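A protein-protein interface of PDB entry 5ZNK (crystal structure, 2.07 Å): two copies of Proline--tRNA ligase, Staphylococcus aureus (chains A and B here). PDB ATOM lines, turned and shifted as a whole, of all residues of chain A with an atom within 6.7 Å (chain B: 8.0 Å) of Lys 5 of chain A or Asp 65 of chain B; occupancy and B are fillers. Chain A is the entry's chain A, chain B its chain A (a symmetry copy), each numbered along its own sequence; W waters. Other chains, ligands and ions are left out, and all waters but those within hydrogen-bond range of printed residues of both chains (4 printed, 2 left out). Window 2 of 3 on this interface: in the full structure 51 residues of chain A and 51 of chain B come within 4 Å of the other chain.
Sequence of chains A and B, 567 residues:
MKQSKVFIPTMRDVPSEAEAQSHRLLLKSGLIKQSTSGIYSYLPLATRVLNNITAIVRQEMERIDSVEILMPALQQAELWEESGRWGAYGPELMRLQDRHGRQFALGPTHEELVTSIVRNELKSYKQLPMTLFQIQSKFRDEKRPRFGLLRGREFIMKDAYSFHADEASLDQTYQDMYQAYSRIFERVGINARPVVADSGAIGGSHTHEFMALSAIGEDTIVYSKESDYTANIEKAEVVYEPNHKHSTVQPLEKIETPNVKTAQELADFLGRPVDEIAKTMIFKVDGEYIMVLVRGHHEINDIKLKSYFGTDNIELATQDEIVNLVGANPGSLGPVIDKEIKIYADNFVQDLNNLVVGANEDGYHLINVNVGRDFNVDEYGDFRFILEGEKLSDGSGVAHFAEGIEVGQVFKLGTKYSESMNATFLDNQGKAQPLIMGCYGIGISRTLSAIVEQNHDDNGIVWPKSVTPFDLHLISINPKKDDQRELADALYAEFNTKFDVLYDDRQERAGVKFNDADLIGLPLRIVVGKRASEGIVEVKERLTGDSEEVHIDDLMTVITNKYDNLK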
ATOM      1  N   MET A   1      -8.466   1.533 -14.579  1.00  0.00           N
ATOM      2  CA  MET A   1      -9.233   2.806 -14.577  1.00  0.00           C
ATOM      3  C   MET A   1      -8.711   3.732 -15.666  1.00  0.00           C
ATOM      4  O   MET A   1      -7.508   3.786 -15.926  1.00  0.00           O
ATOM      5  CB  MET A   1      -9.113   3.522 -13.226  1.00  0.00           C
ATOM      6  CG  MET A   1      -9.931   2.933 -12.091  1.00  0.00           C
ATOM      7  SD  MET A   1     -11.726   3.132 -12.236  1.00  0.00           S
ATOM      8  CE  MET A   1     -11.849   4.793 -12.889  1.00  0.00           C
ATOM      9  N   LYS A   2      -9.633   4.463 -16.286  1.00  0.00           N
ATOM     10  CA  LYS A   2      -9.299   5.541 -17.193  1.00  0.00           C
ATOM     11  C   LYS A   2      -9.019   6.766 -16.342  1.00  0.00           C
ATOM     12  O   LYS A   2      -9.799   7.098 -15.440  1.00  0.00           O
ATOM     13  CB  LYS A   2     -10.441   5.792 -18.166  1.00  0.00           C
ATOM     14  CG  LYS A   2     -10.610   4.667 -19.168  1.00  0.00           C
ATOM     15  CD  LYS A   2     -11.512   5.072 -20.323  1.00  0.00           C
ATOM     16  CE  LYS A   2     -11.413   4.093 -21.483  1.00  0.00           C
ATOM     17  NZ  LYS A   2     -12.152   2.827 -21.216  1.00  0.00           N
ATOM     18  N   GLN A   3      -7.903   7.435 -16.632  1.00  0.00           N
ATOM     19  CA  GLN A   3      -7.436   8.551 -15.819  1.00  0.00           C
ATOM     20  C   GLN A   3      -8.369   9.760 -15.851  1.00  0.00           C
ATOM     21  O   GLN A   3      -8.451  10.507 -14.879  1.00  0.00           O
ATOM     22  CB  GLN A   3      -6.027   8.958 -16.233  1.00  0.00           C
ATOM     23  CG  GLN A   3      -5.320   9.825 -15.205  1.00  0.00           C
ATOM     24  CD  GLN A   3      -3.828   9.929 -15.442  1.00  0.00           C
ATOM     25  OE1 GLN A   3      -3.196   8.978 -15.899  1.00  0.00           O
ATOM     26  NE2 GLN A   3      -3.255  11.081 -15.123  1.00  0.00           N
ATOM     27  N   SER A   4      -9.091   9.923 -16.957  1.00  0.00           N
ATOM     28  CA  SER A   4     -10.151  10.933 -17.080  1.00  0.00           C
ATOM     29  C   SER A   4     -11.255  10.808 -16.014  1.00  0.00           C
ATOM     30  O   SER A   4     -11.973  11.770 -15.758  1.00  0.00           O
ATOM     31  CB  SER A   4     -10.794  10.851 -18.467  1.00  0.00           C
ATOM     32  OG  SER A   4     -11.378   9.578 -18.666  1.00  0.00           O
ATOM     33  N   LYS A   5     -11.398   9.618 -15.430  1.00  0.00           N
ATOM     34  CA  LYS A   5     -12.395   9.357 -14.395  1.00  0.00           C
ATOM     35  C   LYS A   5     -11.829   9.278 -12.963  1.00  0.00           C
ATOM     36  O   LYS A   5     -12.573   9.020 -12.022  1.00  0.00           O
ATOM     37  CB  LYS A   5     -13.168   8.086 -14.777  1.00  0.00           C
ATOM     38  CG  LYS A   5     -14.345   8.381 -15.700  1.00  0.00           C
ATOM     39  CD  LYS A   5     -14.374   7.492 -16.925  1.00  0.00           C
ATOM     40  CE  LYS A   5     -15.413   7.976 -17.929  1.00  0.00           C
ATOM     41  NZ  LYS A   5     -15.041   7.557 -19.309  1.00  0.00           N
ATOM     42  N   VAL A   6     -10.532   9.536 -12.807  1.00  0.00           N
ATOM     43  CA  VAL A   6      -9.862   9.480 -11.509  1.00  0.00           C
ATOM     44  C   VAL A   6      -9.448  10.885 -11.096  1.00  0.00           C
ATOM     45  O   VAL A   6      -8.744  11.566 -11.832  1.00  0.00           O
ATOM     46  CB  VAL A   6      -8.628   8.559 -11.555  1.00  0.00           C
ATOM     47  CG1 VAL A   6      -7.971   8.413 -10.185  1.00  0.00           C
ATOM     48  CG2 VAL A   6      -9.021   7.200 -12.077  1.00  0.00           C
ATOM     49  N   PHE A   7      -9.878  11.300  -9.909  1.00  0.00           N
ATOM     50  CA  PHE A   7      -9.518  12.588  -9.338  1.00  0.00           C
ATOM     51  C   PHE A   7      -8.060  12.570  -8.854  1.00  0.00           C
ATOM     52  O   PHE A   7      -7.725  11.870  -7.893  1.00  0.00           O
ATOM     53  CB  PHE A   7     -10.466  12.915  -8.182  1.00  0.00           C
ATOM     54  CG  PHE A   7     -10.291  14.295  -7.621  1.00  0.00           C
ATOM     55  CD1 PHE A   7     -10.492  15.415  -8.424  1.00  0.00           C
ATOM     56  CD2 PHE A   7      -9.942  14.481  -6.289  1.00  0.00           C
ATOM     57  CE1 PHE A   7     -10.332  16.690  -7.911  1.00  0.00           C
ATOM     58  CE2 PHE A   7      -9.793  15.749  -5.769  1.00  0.00           C
ATOM     59  CZ  PHE A   7      -9.982  16.858  -6.580  1.00  0.00           C
ATOM     60  N   PRO A  44      -7.940   9.511  -4.437  1.00  0.00           N
ATOM     61  CA  PRO A  44      -8.035   8.165  -4.982  1.00  0.00           C
ATOM     62  C   PRO A  44      -6.788   7.298  -4.950  1.00  0.00           C
ATOM     63  O   PRO A  44      -6.865   6.156  -4.523  1.00  0.00           O
ATOM     64  CB  PRO A  44      -8.471   8.427  -6.424  1.00  0.00           C
ATOM     65  CG  PRO A  44      -9.437   9.542  -6.268  1.00  0.00           C
ATOM     66  CD  PRO A  44      -8.780  10.440  -5.235  1.00  0.00           C
ATOM     67  N   TYR A 492      -5.159  -1.435 -23.298  1.00  0.00           N
ATOM     68  CA  TYR A 492      -5.860  -1.336 -22.024  1.00  0.00           C
ATOM     69  C   TYR A 492      -6.651  -2.622 -21.726  1.00  0.00           C
ATOM     70  O   TYR A 492      -6.512  -3.225 -20.657  1.00  0.00           O
ATOM     71  CB  TYR A 492      -6.781  -0.123 -22.030  1.00  0.00           C
ATOM     72  CG  TYR A 492      -7.532   0.091 -20.738  1.00  0.00           C
ATOM     73  CD1 TYR A 492      -6.847   0.222 -19.527  1.00  0.00           C
ATOM     74  CD2 TYR A 492      -8.930   0.185 -20.724  1.00  0.00           C
ATOM     75  CE1 TYR A 492      -7.530   0.437 -18.334  1.00  0.00           C
ATOM     76  CE2 TYR A 492      -9.621   0.399 -19.541  1.00  0.00           C
ATOM     77  CZ  TYR A 492      -8.915   0.525 -18.346  1.00  0.00           C
ATOM     78  OH  TYR A 492      -9.589   0.730 -17.166  1.00  0.00           O
ATOM     79  N   ASP A 505      -6.027   8.561 -20.764  1.00  0.00           N
ATOM     80  CA  ASP A 505      -6.837   8.732 -21.954  1.00  0.00           C
ATOM     81  C   ASP A 505      -7.214  10.195 -22.190  1.00  0.00           C
ATOM     82  O   ASP A 505      -8.036  10.481 -23.053  1.00  0.00           O
ATOM     83  CB  ASP A 505      -8.115   7.900 -21.787  1.00  0.00           C
ATOM     84  CG  ASP A 505      -8.999   8.402 -20.668  1.00  0.00           C
ATOM     85  OD1 ASP A 505      -8.475   8.783 -19.598  1.00  0.00           O
ATOM     86  OD2 ASP A 505     -10.229   8.408 -20.841  1.00  0.00           O
ATOM     87  N   ARG A 506      -6.626  11.116 -21.425  1.00  0.00           N
ATOM     88  CA  ARG A 506      -7.094  12.495 -21.427  1.00  0.00           C
ATOM     89  C   ARG A 506      -6.692  13.209 -22.698  1.00  0.00           C
ATOM     90  O   ARG A 506      -5.664  12.896 -23.311  1.00  0.00           O
ATOM     91  CB  ARG A 506      -6.548  13.267 -20.234  1.00  0.00           C
ATOM     92  CG  ARG A 506      -7.041  12.775 -18.883  1.00  0.00           C
ATOM     93  CD  ARG A 506      -6.372  13.560 -17.776  1.00  0.00           C
ATOM     94  NE  ARG A 506      -4.930  13.329 -17.758  1.00  0.00           N
ATOM     95  CZ  ARG A 506      -4.030  14.072 -17.107  1.00  0.00           C
ATOM     96  NH1 ARG A 506      -4.395  15.132 -16.381  1.00  0.00           N
ATOM     97  NH2 ARG A 506      -2.740  13.747 -17.177  1.00  0.00           N
ATOM     98  N   ARG B  58     -17.070  -2.488  -3.361  1.00  0.00           N
ATOM     99  CA  ARG B  58     -15.948  -1.919  -4.105  1.00  0.00           C
ATOM    100  C   ARG B  58     -15.925  -2.368  -5.581  1.00  0.00           C
ATOM    101  O   ARG B  58     -15.626  -1.562  -6.463  1.00  0.00           O
ATOM    102  CB  ARG B  58     -14.604  -2.226  -3.426  1.00  0.00           C
ATOM    103  CG  ARG B  58     -14.298  -1.348  -2.228  1.00  0.00           C
ATOM    104  CD  ARG B  58     -12.900  -1.613  -1.667  1.00  0.00           C
ATOM    105  NE  ARG B  58     -12.659  -0.701  -0.546  1.00  0.00           N
ATOM    106  CZ  ARG B  58     -12.894  -0.960   0.748  1.00  0.00           C
ATOM    107  NH1 ARG B  58     -13.349  -2.151   1.154  1.00  0.00           N
ATOM    108  NH2 ARG B  58     -12.675  -0.011   1.664  1.00  0.00           N
ATOM    109  N   GLN B  59     -16.226  -3.638  -5.848  1.00  0.00           N
ATOM    110  CA  GLN B  59     -16.290  -4.127  -7.230  1.00  0.00           C
ATOM    111  C   GLN B  59     -17.372  -3.385  -8.009  1.00  0.00           C
ATOM    112  O   GLN B  59     -17.131  -2.907  -9.106  1.00  0.00           O
ATOM    113  CB  GLN B  59     -16.628  -5.612  -7.302  1.00  0.00           C
ATOM    114  CG  GLN B  59     -15.531  -6.594  -6.934  1.00  0.00           C
ATOM    115  CD  GLN B  59     -16.058  -8.031  -6.970  1.00  0.00           C
ATOM    116  OE1 GLN B  59     -16.833  -8.395  -7.873  1.00  0.00           O
ATOM    117  NE2 GLN B  59     -15.680  -8.845  -5.973  1.00  0.00           N
ATOM    118  N   GLU B  60     -18.562  -3.290  -7.429  1.00  0.00           N
ATOM    119  CA  GLU B  60     -19.681  -2.644  -8.119  1.00  0.00           C
ATOM    120  C   GLU B  60     -19.446  -1.150  -8.335  1.00  0.00           C
ATOM    121  O   GLU B  60     -19.879  -0.592  -9.350  1.00  0.00           O
ATOM    122  CB  GLU B  60     -21.012  -2.910  -7.401  1.00  0.00           C
ATOM    123  CG  GLU B  60     -21.396  -4.391  -7.357  1.00  0.00           C
ATOM    124  CD  GLU B  60     -21.662  -5.042  -8.714  1.00  0.00           C
ATOM    125  OE1 GLU B  60     -21.981  -4.356  -9.717  1.00  0.00           O
ATOM    126  OE2 GLU B  60     -21.562  -6.279  -8.781  1.00  0.00           O
ATOM    127  N   MET B  61     -18.729  -0.513  -7.409  1.00  0.00           N
ATOM    128  CA  MET B  61     -18.369   0.890  -7.562  1.00  0.00           C
ATOM    129  C   MET B  61     -17.364   1.070  -8.684  1.00  0.00           C
ATOM    130  O   MET B  61     -17.556   1.923  -9.545  1.00  0.00           O
ATOM    131  CB  MET B  61     -17.843   1.482  -6.249  1.00  0.00           C
ATOM    132  CG  MET B  61     -18.912   1.725  -5.193  1.00  0.00           C
ATOM    133  SD  MET B  61     -20.191   2.925  -5.635  1.00  0.00           S
ATOM    134  CE  MET B  61     -21.493   1.856  -6.252  1.00  0.00           C
ATOM    135  N   GLU B  62     -16.309   0.264  -8.689  1.00  0.00           N
ATOM    136  CA  GLU B  62     -15.327   0.337  -9.774  1.00  0.00           C
ATOM    137  C   GLU B  62     -15.939   0.045 -11.161  1.00  0.00           C
ATOM    138  O   GLU B  62     -15.523   0.637 -12.150  1.00  0.00           O
ATOM    139  CB  GLU B  62     -14.121  -0.583  -9.527  1.00  0.00           C
ATOM    140  CG  GLU B  62     -12.967  -0.231 -10.471  1.00  0.00           C
ATOM    141  CD  GLU B  62     -11.690  -1.010 -10.234  1.00  0.00           C
ATOM    142  OE1 GLU B  62     -11.678  -1.943  -9.401  1.00  0.00           O
ATOM    143  OE2 GLU B  62     -10.682  -0.673 -10.899  1.00  0.00           O
ATOM    144  N   ARG B  63     -16.921  -0.847 -11.221  1.00  0.00           N
ATOM    145  CA  ARG B  63     -17.620  -1.173 -12.475  1.00  0.00           C
ATOM    146  C   ARG B  63     -18.320   0.043 -13.127  1.00  0.00           C
ATOM    147  O   ARG B  63     -18.433   0.110 -14.347  1.00  0.00           O
ATOM    148  CB  ARG B  63     -18.629  -2.295 -12.210  1.00  0.00           C
ATOM    149  CG  ARG B  63     -19.344  -2.877 -13.429  1.00  0.00           C
ATOM    150  CD  ARG B  63     -20.405  -3.877 -12.973  1.00  0.00           C
ATOM    151  NE  ARG B  63     -21.035  -4.618 -14.067  1.00  0.00           N
ATOM    152  CZ  ARG B  63     -21.958  -4.137 -14.907  1.00  0.00           C
ATOM    153  NH1 ARG B  63     -22.386  -2.875 -14.820  1.00  0.00           N
ATOM    154  NH2 ARG B  63     -22.457  -4.925 -15.861  1.00  0.00           N
ATOM    155  N   ILE B  64     -18.769   0.996 -12.315  1.00  0.00           N
ATOM    156  CA  ILE B  64     -19.408   2.213 -12.828  1.00  0.00           C
ATOM    157  C   ILE B  64     -18.512   3.443 -12.719  1.00  0.00           C
ATOM    158  O   ILE B  64     -18.998   4.562 -12.773  1.00  0.00           O
ATOM    159  CB  ILE B  64     -20.792   2.477 -12.177  1.00  0.00           C
ATOM    160  CG1 ILE B  64     -20.682   2.681 -10.655  1.00  0.00           C
ATOM    161  CG2 ILE B  64     -21.738   1.333 -12.519  1.00  0.00           C
ATOM    162  CD1 ILE B  64     -21.951   3.201 -10.013  1.00  0.00           C
ATOM    163  N   ASP B  65     -17.201   3.221 -12.617  1.00  0.00           N
ATOM    164  CA  ASP B  65     -16.203   4.291 -12.462  1.00  0.00           C
ATOM    165  C   ASP B  65     -16.454   5.202 -11.268  1.00  0.00           C
ATOM    166  O   ASP B  65     -16.233   6.402 -11.344  1.00  0.00           O
ATOM    167  CB  ASP B  65     -16.068   5.106 -13.757  1.00  0.00           C
ATOM    168  CG  ASP B  65     -15.592   4.273 -14.915  1.00  0.00           C
ATOM    169  OD1 ASP B  65     -14.687   3.436 -14.723  1.00  0.00           O
ATOM    170  OD2 ASP B  65     -16.115   4.453 -16.028  1.00  0.00           O
ATOM    171  N   SER B  66     -16.911   4.625 -10.161  1.00  0.00           N
ATOM    172  CA  SER B  66     -16.995   5.361  -8.892  1.00  0.00           C
ATOM    173  C   SER B  66     -15.683   5.081  -8.156  1.00  0.00           C
ATOM    174  O   SER B  66     -15.354   3.933  -7.903  1.00  0.00           O
ATOM    175  CB  SER B  66     -18.194   4.919  -8.081  1.00  0.00           C
ATOM    176  OG  SER B  66     -18.290   5.619  -6.839  1.00  0.00           O
ATOM    177  N   VAL B  67     -14.943   6.137  -7.825  1.00  0.00           N
ATOM    178  CA  VAL B  67     -13.582   6.007  -7.332  1.00  0.00           C
ATOM    179  C   VAL B  67     -13.444   6.233  -5.832  1.00  0.00           C
ATOM    180  O   VAL B  67     -13.887   7.247  -5.308  1.00  0.00           O
ATOM    181  CB  VAL B  67     -12.668   6.978  -8.101  1.00  0.00           C
ATOM    182  CG1 VAL B  67     -11.224   6.780  -7.691  1.00  0.00           C
ATOM    183  CG2 VAL B  67     -12.807   6.720  -9.596  1.00  0.00           C
ATOM    184  N   GLU B  68     -12.758   5.310  -5.157  1.00  0.00           N
ATOM    185  CA  GLU B  68     -12.693   5.323  -3.703  1.00  0.00           C
ATOM    186  C   GLU B  68     -11.784   6.411  -3.157  1.00  0.00           C
ATOM    187  O   GLU B  68     -10.713   6.669  -3.716  1.00  0.00           O
ATOM    188  CB  GLU B  68     -12.281   3.969  -3.127  1.00  0.00           C
ATOM    189  CG  GLU B  68     -12.687   3.856  -1.666  1.00  0.00           C
ATOM    190  CD  GLU B  68     -12.196   2.619  -0.990  1.00  0.00           C
ATOM    191  OE1 GLU B  68     -11.623   1.747  -1.661  1.00  0.00           O
ATOM    192  OE2 GLU B  68     -12.412   2.515   0.240  1.00  0.00           O
ATOM    193  N   LYS B 126     -14.174  19.609 -19.169  1.00  0.00           N
ATOM    194  CA  LYS B 126     -13.358  18.505 -19.674  1.00  0.00           C
ATOM    195  C   LYS B 126     -13.038  17.435 -18.621  1.00  0.00           C
ATOM    196  O   LYS B 126     -12.751  16.298 -18.971  1.00  0.00           O
ATOM    197  CB  LYS B 126     -12.044  19.039 -20.274  1.00  0.00           C
ATOM    198  CG  LYS B 126     -12.201  19.955 -21.483  1.00  0.00           C
ATOM    199  N   GLN B 127     -13.077  17.800 -17.342  1.00  0.00           N
ATOM    200  CA  GLN B 127     -12.836  16.853 -16.246  1.00  0.00           C
ATOM    201  C   GLN B 127     -14.099  16.150 -15.708  1.00  0.00           C
ATOM    202  O   GLN B 127     -14.005  15.341 -14.777  1.00  0.00           O
ATOM    203  CB  GLN B 127     -12.159  17.576 -15.081  1.00  0.00           C
ATOM    204  CG  GLN B 127     -10.912  18.360 -15.446  1.00  0.00           C
ATOM    205  CD  GLN B 127     -10.462  19.237 -14.300  1.00  0.00           C
ATOM    206  OE1 GLN B 127     -10.796  20.419 -14.247  1.00  0.00           O
ATOM    207  NE2 GLN B 127      -9.744  18.651 -13.351  1.00  0.00           N
ATOM    208  N   LEU B 128     -15.263  16.471 -16.268  1.00  0.00           N
ATOM    209  CA  LEU B 128     -16.542  15.977 -15.753  1.00  0.00           C
ATOM    210  C   LEU B 128     -17.088  14.932 -16.714  1.00  0.00           C
ATOM    211  O   LEU B 128     -16.861  15.062 -17.904  1.00  0.00           O
ATOM    212  CB  LEU B 128     -17.531  17.132 -15.565  1.00  0.00           C
ATOM    213  CG  LEU B 128     -17.045  18.235 -14.607  1.00  0.00           C
ATOM    214  CD1 LEU B 128     -17.999  19.422 -14.604  1.00  0.00           C
ATOM    215  CD2 LEU B 128     -16.846  17.719 -13.186  1.00  0.00           C
ATOM    216  N   PRO B 129     -17.786  13.896 -16.228  1.00  0.00           N
ATOM    217  CA  PRO B 129     -18.161  13.734 -14.821  1.00  0.00           C
ATOM    218  C   PRO B 129     -17.102  13.038 -13.947  1.00  0.00           C
ATOM    219  O   PRO B 129     -16.170  12.392 -14.452  1.00  0.00           O
ATOM    220  CB  PRO B 129     -19.407  12.870 -14.911  1.00  0.00           C
ATOM    221  CG  PRO B 129     -19.145  11.997 -16.098  1.00  0.00           C
ATOM    222  CD  PRO B 129     -18.360  12.829 -17.069  1.00  0.00           C
ATOM    223  N   MET B 130     -17.284  13.187 -12.638  1.00  0.00           N
ATOM    224  CA  MET B 130     -16.402  12.618 -11.630  1.00  0.00           C
ATOM    225  C   MET B 130     -17.267  12.066 -10.499  1.00  0.00           C
ATOM    226  O   MET B 130     -18.141  12.767 -10.005  1.00  0.00           O
ATOM    227  CB  MET B 130     -15.481  13.716 -11.099  1.00  0.00           C
ATOM    228  CG  MET B 130     -14.552  13.314  -9.956  1.00  0.00           C
ATOM    229  SD  MET B 130     -13.440  11.986 -10.421  1.00  0.00           S
ATOM    230  CE  MET B 130     -12.428  12.858 -11.646  1.00  0.00           C
ATOM    231  N   THR B 131     -16.993  10.827 -10.086  1.00  0.00           N
ATOM    232  CA  THR B 131     -17.722  10.158  -9.009  1.00  0.00           C
ATOM    233  C   THR B 131     -16.737   9.621  -7.977  1.00  0.00           C
ATOM    234  O   THR B 131     -15.781   8.915  -8.314  1.00  0.00           O
ATOM    235  CB  THR B 131     -18.605   9.014  -9.547  1.00  0.00           C
ATOM    236  OG1 THR B 131     -19.529   9.544 -10.491  1.00  0.00           O
ATOM    237  CG2 THR B 131     -19.418   8.367  -8.438  1.00  0.00           C
ATOM    238  N   LEU B 132     -16.989   9.973  -6.719  1.00  0.00           N
ATOM    239  CA  LEU B 132     -16.125   9.622  -5.601  1.00  0.00           C
ATOM    240  C   LEU B 132     -16.964   8.938  -4.515  1.00  0.00           C
ATOM    241  O   LEU B 132     -18.114   9.318  -4.295  1.00  0.00           O
ATOM    242  CB  LEU B 132     -15.495  10.868  -5.022  1.00  0.00           C
ATOM    243  CG  LEU B 132     -14.657  11.737  -5.971  1.00  0.00           C
ATOM    244  CD1 LEU B 132     -14.320  13.062  -5.291  1.00  0.00           C
ATOM    245  CD2 LEU B 132     -13.386  11.021  -6.405  1.00  0.00           C
ATOM    246  N   PHE B 133     -16.390   7.937  -3.850  1.00  0.00           N
ATOM    247  CA  PHE B 133     -17.075   7.276  -2.751  1.00  0.00           C
ATOM    248  C   PHE B 133     -16.107   6.889  -1.634  1.00  0.00           C
ATOM    249  O   PHE B 133     -14.916   6.721  -1.855  1.00  0.00           O
ATOM    250  CB  PHE B 133     -17.870   6.067  -3.264  1.00  0.00           C
ATOM    251  CG  PHE B 133     -17.064   4.827  -3.389  1.00  0.00           C
ATOM    252  CD1 PHE B 133     -16.287   4.599  -4.516  1.00  0.00           C
ATOM    253  CD2 PHE B 133     -17.049   3.885  -2.359  1.00  0.00           C
ATOM    254  CE1 PHE B 133     -15.510   3.454  -4.609  1.00  0.00           C
ATOM    255  CE2 PHE B 133     -16.285   2.741  -2.451  1.00  0.00           C
ATOM    256  CZ  PHE B 133     -15.520   2.525  -3.582  1.00  0.00           C
ATOM    257  N   TYR B 161     -20.528  10.549  -4.118  1.00  0.00           N
ATOM    258  CA  TYR B 161     -20.840  11.899  -4.546  1.00  0.00           C
ATOM    259  C   TYR B 161     -20.369  12.041  -5.981  1.00  0.00           C
ATOM    260  O   TYR B 161     -19.234  11.665  -6.294  1.00  0.00           O
ATOM    261  CB  TYR B 161     -20.140  12.921  -3.638  1.00  0.00           C
ATOM    262  CG  TYR B 161     -20.419  12.682  -2.180  1.00  0.00           C
ATOM    263  CD1 TYR B 161     -19.605  11.851  -1.431  1.00  0.00           C
ATOM    264  CD2 TYR B 161     -21.517  13.264  -1.555  1.00  0.00           C
ATOM    265  CE1 TYR B 161     -19.856  11.616  -0.096  1.00  0.00           C
ATOM    266  CE2 TYR B 161     -21.797  13.029  -0.213  1.00  0.00           C
ATOM    267  CZ  TYR B 161     -20.972  12.196   0.510  1.00  0.00           C
ATOM    268  OH  TYR B 161     -21.235  11.946   1.842  1.00  0.00           O
ATOM    269  N   THR B 173     -25.346   8.983 -14.309  1.00  0.00           N
ATOM    270  CA  THR B 173     -24.687   8.452 -13.103  1.00  0.00           C
ATOM    271  C   THR B 173     -25.705   7.960 -12.063  1.00  0.00           C
ATOM    272  O   THR B 173     -25.489   6.928 -11.450  1.00  0.00           O
ATOM    273  CB  THR B 173     -23.714   9.462 -12.481  1.00  0.00           C
ATOM    274  OG1 THR B 173     -22.644   9.668 -13.395  1.00  0.00           O
ATOM    275  CG2 THR B 173     -23.093   8.933 -11.194  1.00  0.00           C
ATOM    276  N   ASP B 176     -26.720   4.619 -13.238  1.00  0.00           N
ATOM    277  CA  ASP B 176     -25.611   3.701 -12.956  1.00  0.00           C
ATOM    278  C   ASP B 176     -25.601   3.250 -11.496  1.00  0.00           C
ATOM    279  O   ASP B 176     -25.446   2.067 -11.191  1.00  0.00           O
ATOM    280  CB  ASP B 176     -24.261   4.373 -13.269  1.00  0.00           C
ATOM    281  CG  ASP B 176     -24.009   4.564 -14.762  1.00  0.00           C
ATOM    282  OD1 ASP B 176     -24.631   3.872 -15.590  1.00  0.00           O
ATOM    283  OD2 ASP B 176     -23.152   5.402 -15.113  1.00  0.00           O
ATOM    284  N   MET B 177     -25.767   4.210 -10.596  1.00  0.00           N
ATOM    285  CA  MET B 177     -25.798   3.926  -9.159  1.00  0.00           C
ATOM    286  C   MET B 177     -27.005   3.079  -8.777  1.00  0.00           C
ATOM    287  O   MET B 177     -26.886   2.163  -7.977  1.00  0.00           O
ATOM    288  CB  MET B 177     -25.793   5.219  -8.352  1.00  0.00           C
ATOM    289  CG  MET B 177     -24.455   5.907  -8.313  1.00  0.00           C
ATOM    290  SD  MET B 177     -23.359   5.190  -7.063  1.00  0.00           S
ATOM    291  CE  MET B 177     -21.890   6.125  -7.424  1.00  0.00           C
HETATM  292  O   HOH W   1     -11.636  14.280 -14.477  1.00  0.00           O
HETATM  293  O   HOH W   2     -14.743  12.253 -16.854  1.00  0.00           O
HETATM  294  O   HOH W   3     -12.243   3.782 -16.261  1.00  0.00           O
HETATM  295  O   HOH W   4      -9.255   4.976  -5.186  1.00  0.00           O
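N of Phe 7 of chain A lies close to SD of Met 130 of chain B (3.7 Å).
The side-chain sulfur (SD) of Met 130 of chain B sits close to the backbone carbonyl oxygen (O) of Lys 5 of chain A.
The side-chain hydroxyl (OH) of Tyr 492 of chain A sits at hydrogen-bond distance from the backbone NH (N) of Met 1 of chain A.
The guanidinium group of Arg 58 of chain B is in salt-bridge range of the side-chain carboxylate of Glu 68 of chain B (2.9 Å).
The backbone carbonyl oxygen (O) of Leu 132 of chain B lies within hydrogen-bond range of the backbone NH (N) of Tyr 161 of chain B.
Among the printed residues, pairs that only touch across the chains: Pro 44 of chain A with Glu 68 of chain B (3.3 Å), Lys 5 of chain A with Val 67 of chain B (3.4 Å), Pro 44 of chain A with Val 67 of chain B (3.4 Å), Lys 5 of chain A with Asp 65 of chain B (3.6 Å), Val 6 of chain A with Met 130 of chain B (3.6 Å), Met 1 of chain A with Asp 65 of chain B (3.6 Å), Met 1 of chain A with Glu 62 of chain B (3.9 Å), Phe 7 of chain A with Leu 132 of chain B (3.9 Å) and Met 1 of chain A with Val 67 of chain B (3.9 Å).
Of the printed residues of chain B, Met 1 of chain A touches Glu 62, Asp 65 and Val 67.
No residue of chain B comes within 4 Å of Ser 4 of chain A.
Lys 5 of chain A touches just these residues of chain B: Asp 65, Val 67 and Met 130.
Of the printed residues of chain B, Pro 44 of chain A touches Val 67 (3.4 Å) and Glu 68 (3.3 Å).
Of the printed residues of chain A, Asp 65 of chain B touches Met 1 (3.6 Å) and Lys 5 (3.6 Å).
Of the printed residues of chain A, Glu 68 of chain B touches Pro 44 (3.3 Å).
Of the printed residues of chain A, Leu 132 of chain B touches Phe 7.
Tyr 161 of chain B touches none of the printed residues of chain A.
The nearest printed residue of chain A that does not touch Asp 65 of chain B is Lys 2 of chain A (5.4 Å).
The nearest printed residue of chain B that does not touch Val 6 of chain A is Val 67 of chain B (4.4 Å).
Of the 23 printed residues of chain B, 6 touch a printed residue of chain A.
Hydrophobic or aromatic side chains of chain B that line the printed part of chain A: Val 67, Met 130 and Leu 132.
Of the 11 printed residues of chain A, 5 touch a printed residue of chain B.
Hydrophobic or aromatic side chains of chain A within 4 Å of the printed part of chain B: Met 1, Phe 7 and Pro 44.
Among the printed residues, 11 pairs touch across the chains.
No position is printed for both chains.
Water W1 lies within hydrogen-bond range of the backbone carbonyl oxygen of Gln 127 of chain B (2.6 Å) and the backbone carbonyl oxygen of Ser 4 of chain A (2.8 Å).
Water W4 lies within hydrogen-bond range of O of Glu 68 of chain B and O of Pro 44 of chain A.
Water W3 bridges N of Lys 2 of chain A (2.7 Å) and OD1 of Asp 65 of chain B (2.9 Å).
Water W2 lies within hydrogen-bond range of the backbone carbonyl oxygen (O) of Pro 129 of chain B (2.8 Å) and the backbone carbonyl oxygen (O) of Ser 4 of chain A (3.0 Å).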
